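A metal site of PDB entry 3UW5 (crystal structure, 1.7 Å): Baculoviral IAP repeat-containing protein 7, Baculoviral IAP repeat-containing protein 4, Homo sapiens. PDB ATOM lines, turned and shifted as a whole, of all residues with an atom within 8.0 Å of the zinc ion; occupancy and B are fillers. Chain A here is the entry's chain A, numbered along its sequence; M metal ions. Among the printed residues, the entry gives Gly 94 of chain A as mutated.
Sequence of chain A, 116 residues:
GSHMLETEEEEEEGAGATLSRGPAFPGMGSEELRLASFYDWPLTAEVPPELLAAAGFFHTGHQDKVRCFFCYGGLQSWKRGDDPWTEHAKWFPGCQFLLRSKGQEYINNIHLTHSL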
ATOM      1  N   ALA A  55      -1.181  24.530   2.327  1.00  0.00           N
ATOM      2  CA  ALA A  55      -1.217  23.984   0.976  1.00  0.00           C
ATOM      3  C   ALA A  55      -2.225  22.845   0.783  1.00  0.00           C
ATOM      4  O   ALA A  55      -2.241  22.225  -0.271  1.00  0.00           O
ATOM      5  CB  ALA A  55       0.176  23.522   0.570  1.00  0.00           C
ATOM      6  N   GLY A  56      -3.059  22.586   1.793  1.00  0.00           N
ATOM      7  CA  GLY A  56      -4.146  21.617   1.681  1.00  0.00           C
ATOM      8  C   GLY A  56      -3.828  20.239   2.230  1.00  0.00           C
ATOM      9  O   GLY A  56      -4.684  19.354   2.219  1.00  0.00           O
ATOM     10  N   PHE A  57      -2.618  20.071   2.752  1.00  0.00           N
ATOM     11  CA  PHE A  57      -2.139  18.745   3.158  1.00  0.00           C
ATOM     12  C   PHE A  57      -2.399  18.451   4.623  1.00  0.00           C
ATOM     13  O   PHE A  57      -2.286  19.343   5.477  1.00  0.00           O
ATOM     14  CB  PHE A  57      -0.644  18.602   2.879  1.00  0.00           C
ATOM     15  CG  PHE A  57      -0.291  18.693   1.421  1.00  0.00           C
ATOM     16  CD1 PHE A  57      -0.720  17.720   0.524  1.00  0.00           C
ATOM     17  CD2 PHE A  57       0.475  19.749   0.944  1.00  0.00           C
ATOM     18  CE1 PHE A  57      -0.408  17.808  -0.817  1.00  0.00           C
ATOM     19  CE2 PHE A  57       0.806  19.827  -0.398  1.00  0.00           C
ATOM     20  CZ  PHE A  57       0.362  18.863  -1.281  1.00  0.00           C
ATOM     21  N   ARG A  67      -1.542  13.853   2.540  1.00  0.00           N
ATOM     22  CA  ARG A  67      -2.510  13.907   1.456  1.00  0.00           C
ATOM     23  C   ARG A  67      -3.217  15.244   1.426  1.00  0.00           C
ATOM     24  O   ARG A  67      -3.431  15.867   2.465  1.00  0.00           O
ATOM     25  CB  ARG A  67      -3.573  12.815   1.612  1.00  0.00           C
ATOM     26  CG  ARG A  67      -3.152  11.433   1.154  1.00  0.00           C
ATOM     27  CD  ARG A  67      -4.368  10.517   1.169  1.00  0.00           C
ATOM     28  NE  ARG A  67      -4.023   9.108   1.006  1.00  0.00           N
ATOM     29  CZ  ARG A  67      -3.824   8.505  -0.162  1.00  0.00           C
ATOM     30  NH1 ARG A  67      -3.902   9.185  -1.310  1.00  0.00           N
ATOM     31  NH2 ARG A  67      -3.529   7.213  -0.176  1.00  0.00           N
ATOM     32  N   CYS A  68      -3.598  15.680   0.227  1.00  0.00           N
ATOM     33  CA  CYS A  68      -4.446  16.854   0.082  1.00  0.00           C
ATOM     34  C   CYS A  68      -5.887  16.481   0.403  1.00  0.00           C
ATOM     35  O   CYS A  68      -6.382  15.454  -0.068  1.00  0.00           O
ATOM     36  CB  CYS A  68      -4.347  17.389  -1.337  1.00  0.00           C
ATOM     37  SG  CYS A  68      -5.493  18.736  -1.726  1.00  0.00           S
ATOM     38  N   PHE A  69      -6.568  17.314   1.186  1.00  0.00           N
ATOM     39  CA  PHE A  69      -7.963  17.034   1.553  1.00  0.00           C
ATOM     40  C   PHE A  69      -8.881  17.107   0.329  1.00  0.00           C
ATOM     41  O   PHE A  69      -9.950  16.486   0.319  1.00  0.00           O
ATOM     42  CB  PHE A  69      -8.458  18.012   2.623  1.00  0.00           C
ATOM     43  CG  PHE A  69      -8.915  19.336   2.062  1.00  0.00           C
ATOM     44  CD1 PHE A  69      -7.996  20.345   1.801  1.00  0.00           C
ATOM     45  CD2 PHE A  69     -10.248  19.552   1.779  1.00  0.00           C
ATOM     46  CE1 PHE A  69      -8.417  21.554   1.282  1.00  0.00           C
ATOM     47  CE2 PHE A  69     -10.676  20.751   1.238  1.00  0.00           C
ATOM     48  CZ  PHE A  69      -9.755  21.762   1.000  1.00  0.00           C
ATOM     49  N   PHE A  70      -8.492  17.868  -0.690  1.00  0.00           N
ATOM     50  CA  PHE A  70      -9.367  18.095  -1.830  1.00  0.00           C
ATOM     51  C   PHE A  70      -9.190  17.060  -2.940  1.00  0.00           C
ATOM     52  O   PHE A  70     -10.161  16.433  -3.350  1.00  0.00           O
ATOM     53  CB  PHE A  70      -9.208  19.504  -2.399  1.00  0.00           C
ATOM     54  CG  PHE A  70     -10.372  19.911  -3.249  1.00  0.00           C
ATOM     55  CD1 PHE A  70     -10.468  19.499  -4.568  1.00  0.00           C
ATOM     56  CD2 PHE A  70     -11.419  20.650  -2.698  1.00  0.00           C
ATOM     57  CE1 PHE A  70     -11.562  19.834  -5.332  1.00  0.00           C
ATOM     58  CE2 PHE A  70     -12.516  20.998  -3.466  1.00  0.00           C
ATOM     59  CZ  PHE A  70     -12.591  20.587  -4.778  1.00  0.00           C
ATOM     60  N   CYS A  71      -7.971  16.923  -3.445  1.00  0.00           N
ATOM     61  CA  CYS A  71      -7.695  15.984  -4.545  1.00  0.00           C
ATOM     62  C   CYS A  71      -7.252  14.604  -4.062  1.00  0.00           C
ATOM     63  O   CYS A  71      -7.198  13.678  -4.872  1.00  0.00           O
ATOM     64  CB  CYS A  71      -6.657  16.570  -5.516  1.00  0.00           C
ATOM     65  SG  CYS A  71      -4.990  16.769  -4.867  1.00  0.00           S
ATOM     66  N   TYR A  72      -6.953  14.477  -2.764  1.00  0.00           N
ATOM     67  CA  TYR A  72      -6.472  13.238  -2.118  1.00  0.00           C
ATOM     68  C   TYR A  72      -5.082  12.802  -2.619  1.00  0.00           C
ATOM     69  O   TYR A  72      -4.657  11.670  -2.368  1.00  0.00           O
ATOM     70  CB  TYR A  72      -7.490  12.084  -2.279  1.00  0.00           C
ATOM     71  CG  TYR A  72      -7.663  11.212  -1.038  1.00  0.00           C
ATOM     72  CD1 TYR A  72      -8.096  11.756   0.165  1.00  0.00           C
ATOM     73  CD2 TYR A  72      -7.450   9.834  -1.090  1.00  0.00           C
ATOM     74  CE1 TYR A  72      -8.280  10.958   1.296  1.00  0.00           C
ATOM     75  CE2 TYR A  72      -7.646   9.031   0.039  1.00  0.00           C
ATOM     76  CZ  TYR A  72      -8.060   9.597   1.220  1.00  0.00           C
ATOM     77  OH  TYR A  72      -8.262   8.821   2.362  1.00  0.00           O
ATOM     78  N   GLY A  73      -4.381  13.694  -3.304  1.00  0.00           N
ATOM     79  CA  GLY A  73      -3.041  13.407  -3.806  1.00  0.00           C
ATOM     80  C   GLY A  73      -2.114  13.179  -2.626  1.00  0.00           C
ATOM     81  O   GLY A  73      -2.104  13.962  -1.682  1.00  0.00           O
ATOM     82  N   GLY A  74      -1.345  12.085  -2.670  1.00  0.00           N
ATOM     83  CA  GLY A  74      -0.445  11.728  -1.586  1.00  0.00           C
ATOM     84  C   GLY A  74       1.010  11.981  -1.926  1.00  0.00           C
ATOM     85  O   GLY A  74       1.470  11.559  -2.987  1.00  0.00           O
ATOM     86  N   TRP A  85       3.323  24.112  -1.660  1.00  0.00           N
ATOM     87  CA  TRP A  85       2.530  24.579  -2.790  1.00  0.00           C
ATOM     88  C   TRP A  85       3.132  24.198  -4.118  1.00  0.00           C
ATOM     89  O   TRP A  85       2.424  23.768  -5.032  1.00  0.00           O
ATOM     90  CB  TRP A  85       2.327  26.097  -2.748  1.00  0.00           C
ATOM     91  CG  TRP A  85       1.134  26.571  -1.962  1.00  0.00           C
ATOM     92  CD1 TRP A  85       1.100  27.558  -0.976  1.00  0.00           C
ATOM     93  CD2 TRP A  85      -0.262  26.125  -2.096  1.00  0.00           C
ATOM     94  NE1 TRP A  85      -0.182  27.735  -0.503  1.00  0.00           N
ATOM     95  CE2 TRP A  85      -1.035  26.907  -1.136  1.00  0.00           C
ATOM     96  CE3 TRP A  85      -0.913  25.194  -2.884  1.00  0.00           C
ATOM     97  CZ2 TRP A  85      -2.408  26.743  -0.987  1.00  0.00           C
ATOM     98  CZ3 TRP A  85      -2.293  25.034  -2.716  1.00  0.00           C
ATOM     99  CH2 TRP A  85      -3.017  25.800  -1.801  1.00  0.00           C
ATOM    100  N   HIS A  88       2.565  20.578  -4.666  1.00  0.00           N
ATOM    101  CA  HIS A  88       1.143  20.387  -4.983  1.00  0.00           C
ATOM    102  C   HIS A  88       0.900  20.629  -6.444  1.00  0.00           C
ATOM    103  O   HIS A  88       0.226  19.844  -7.114  1.00  0.00           O
ATOM    104  CB  HIS A  88       0.290  21.345  -4.139  1.00  0.00           C
ATOM    105  CG  HIS A  88      -1.115  20.839  -3.848  1.00  0.00           C
ATOM    106  ND1 HIS A  88      -1.779  21.188  -2.729  1.00  0.00           N
ATOM    107  CD2 HIS A  88      -1.977  20.008  -4.571  1.00  0.00           C
ATOM    108  CE1 HIS A  88      -2.992  20.607  -2.722  1.00  0.00           C
ATOM    109  NE2 HIS A  88      -3.118  19.890  -3.842  1.00  0.00           N
ATOM    110  N   ALA A  89       1.451  21.723  -6.961  1.00  0.00           N
ATOM    111  CA  ALA A  89       1.261  22.112  -8.365  1.00  0.00           C
ATOM    112  C   ALA A  89       2.037  21.226  -9.330  1.00  0.00           C
ATOM    113  O   ALA A  89       1.577  20.979 -10.446  1.00  0.00           O
ATOM    114  CB  ALA A  89       1.645  23.574  -8.565  1.00  0.00           C
ATOM    115  N   PHE A  92       0.016  17.455  -8.737  1.00  0.00           N
ATOM    116  CA  PHE A  92      -1.440  17.422  -8.846  1.00  0.00           C
ATOM    117  C   PHE A  92      -1.990  18.735  -9.425  1.00  0.00           C
ATOM    118  O   PHE A  92      -2.816  19.403  -8.802  1.00  0.00           O
ATOM    119  CB  PHE A  92      -2.073  17.114  -7.493  1.00  0.00           C
ATOM    120  CG  PHE A  92      -1.373  16.022  -6.735  1.00  0.00           C
ATOM    121  CD1 PHE A  92      -1.373  14.714  -7.215  1.00  0.00           C
ATOM    122  CD2 PHE A  92      -0.721  16.292  -5.548  1.00  0.00           C
ATOM    123  CE1 PHE A  92      -0.724  13.710  -6.518  1.00  0.00           C
ATOM    124  CE2 PHE A  92      -0.071  15.298  -4.843  1.00  0.00           C
ATOM    125  CZ  PHE A  92      -0.075  14.003  -5.327  1.00  0.00           C
ATOM    126  N   PRO A  93      -1.560  19.099 -10.643  1.00  0.00           N
ATOM    127  CA  PRO A  93      -1.913  20.392 -11.226  1.00  0.00           C
ATOM    128  C   PRO A  93      -3.413  20.604 -11.489  1.00  0.00           C
ATOM    129  O   PRO A  93      -3.828  21.748 -11.674  1.00  0.00           O
ATOM    130  CB  PRO A  93      -1.144  20.410 -12.545  1.00  0.00           C
ATOM    131  CG  PRO A  93      -0.935  18.977 -12.878  1.00  0.00           C
ATOM    132  CD  PRO A  93      -0.722  18.299 -11.555  1.00  0.00           C
ATOM    133  N   GLY A  94      -4.207  19.532 -11.485  1.00  0.00           N
ATOM    134  CA  GLY A  94      -5.653  19.629 -11.721  1.00  0.00           C
ATOM    135  C   GLY A  94      -6.492  19.830 -10.472  1.00  0.00           C
ATOM    136  O   GLY A  94      -7.714  19.919 -10.553  1.00  0.00           O
ATOM    137  N   CYS A  95      -5.848  19.899  -9.312  1.00  0.00           N
ATOM    138  CA  CYS A  95      -6.557  20.059  -8.051  1.00  0.00           C
ATOM    139  C   CYS A  95      -7.272  21.408  -8.000  1.00  0.00           C
ATOM    140  O   CYS A  95      -6.656  22.449  -8.220  1.00  0.00           O
ATOM    141  CB  CYS A  95      -5.575  19.982  -6.891  1.00  0.00           C
ATOM    142  SG  CYS A  95      -6.337  20.265  -5.288  1.00  0.00           S
ATOM    143  N   GLN A  96      -8.557  21.393  -7.685  1.00  0.00           N
ATOM    144  CA  GLN A  96      -9.352  22.620  -7.684  1.00  0.00           C
ATOM    145  C   GLN A  96      -9.100  23.517  -6.479  1.00  0.00           C
ATOM    146  O   GLN A  96      -9.248  24.726  -6.580  1.00  0.00           O
ATOM    147  CB  GLN A  96     -10.842  22.299  -7.828  1.00  0.00           C
ATOM    148  CG  GLN A  96     -11.185  21.682  -9.179  1.00  0.00           C
ATOM    149  CD  GLN A  96     -10.843  22.588 -10.338  1.00  0.00           C
ATOM    150  OE1 GLN A  96     -11.500  23.616 -10.554  1.00  0.00           O
ATOM    151  NE2 GLN A  96      -9.800  22.238 -11.089  1.00  0.00           N
ATOM    152  N   PHE A  97      -8.724  22.921  -5.350  1.00  0.00           N
ATOM    153  CA  PHE A  97      -8.277  23.694  -4.199  1.00  0.00           C
ATOM    154  C   PHE A  97      -6.994  24.471  -4.526  1.00  0.00           C
ATOM    155  O   PHE A  97      -6.875  25.650  -4.200  1.00  0.00           O
ATOM    156  CB  PHE A  97      -8.043  22.795  -2.986  1.00  0.00           C
ATOM    157  CG  PHE A  97      -7.465  23.515  -1.810  1.00  0.00           C
ATOM    158  CD1 PHE A  97      -8.253  24.356  -1.045  1.00  0.00           C
ATOM    159  CD2 PHE A  97      -6.131  23.360  -1.467  1.00  0.00           C
ATOM    160  CE1 PHE A  97      -7.722  25.036   0.039  1.00  0.00           C
ATOM    161  CE2 PHE A  97      -5.589  24.034  -0.389  1.00  0.00           C
ATOM    162  CZ  PHE A  97      -6.390  24.870   0.374  1.00  0.00           C
ATOM    163  N   LEU A  98      -6.041  23.795  -5.147  1.00  0.00           N
ATOM    164  CA  LEU A  98      -4.825  24.434  -5.646  1.00  0.00           C
ATOM    165  C   LEU A  98      -5.176  25.595  -6.575  1.00  0.00           C
ATOM    166  O   LEU A  98      -4.659  26.709  -6.401  1.00  0.00           O
ATOM    167  CB  LEU A  98      -3.952  23.419  -6.381  1.00  0.00           C
ATOM    168  CG  LEU A  98      -2.758  23.942  -7.184  1.00  0.00           C
ATOM    169  CD1 LEU A  98      -1.693  24.509  -6.259  1.00  0.00           C
ATOM    170  CD2 LEU A  98      -2.197  22.803  -8.038  1.00  0.00           C
ATOM    171  N   LEU A  99      -6.030  25.343  -7.563  1.00  0.00           N
ATOM    172  CA  LEU A  99      -6.427  26.379  -8.519  1.00  0.00           C
ATOM    173  C   LEU A  99      -7.065  27.576  -7.826  1.00  0.00           C
ATOM    174  O   LEU A  99      -6.663  28.712  -8.056  1.00  0.00           O
ATOM    175  CB  LEU A  99      -7.384  25.814  -9.571  1.00  0.00           C
ATOM    176  CG  LEU A  99      -7.980  26.810 -10.574  1.00  0.00           C
ATOM    177  CD1 LEU A  99      -6.887  27.569 -11.309  1.00  0.00           C
ATOM    178  CD2 LEU A  99      -8.888  26.093 -11.548  1.00  0.00           C
HETATM  179 ZN    ZN M   1      -4.958  18.914  -3.982  1.00  0.00          ZN
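The backbone NH (N) of Cys 68 lies within hydrogen-bond range of the backbone carbonyl oxygen (O) of Gly 73, 3.0 Å away. The backbone NH (N) of Phe 70 sits close to the side-chain sulfur (SG) of Cys 68 (3.3 Å). The backbone NH (N) of Phe 97 sits close to the side-chain sulfur (SG) of Cys 95, at 3.6 Å. The backbone NH of Gly 73 sits close to the side-chain sulfur of Cys 71. The backbone NH (N) of Leu 98 lies close to the side-chain sulfur (SG) of Cys 95, 3.5 Å away. The backbone carbonyl oxygen of Ala 55 sits at hydrogen-bond distance from a ring nitrogen (ND1) of His 88.
The nearest printed residue that does not touch the zinc ion is Phe 70 (4.6 Å).
The zinc ion is bound by a ring nitrogen (NE2) of His 88 (2.1 Å), the side-chain sulfur of Cys 71 (2.3 Å), the side-chain sulfur of Cys 68 (2.3 Å) and the side-chain sulfur of Cys 95 (2.3 Å). The zinc ion has four donor atoms within binding distance.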
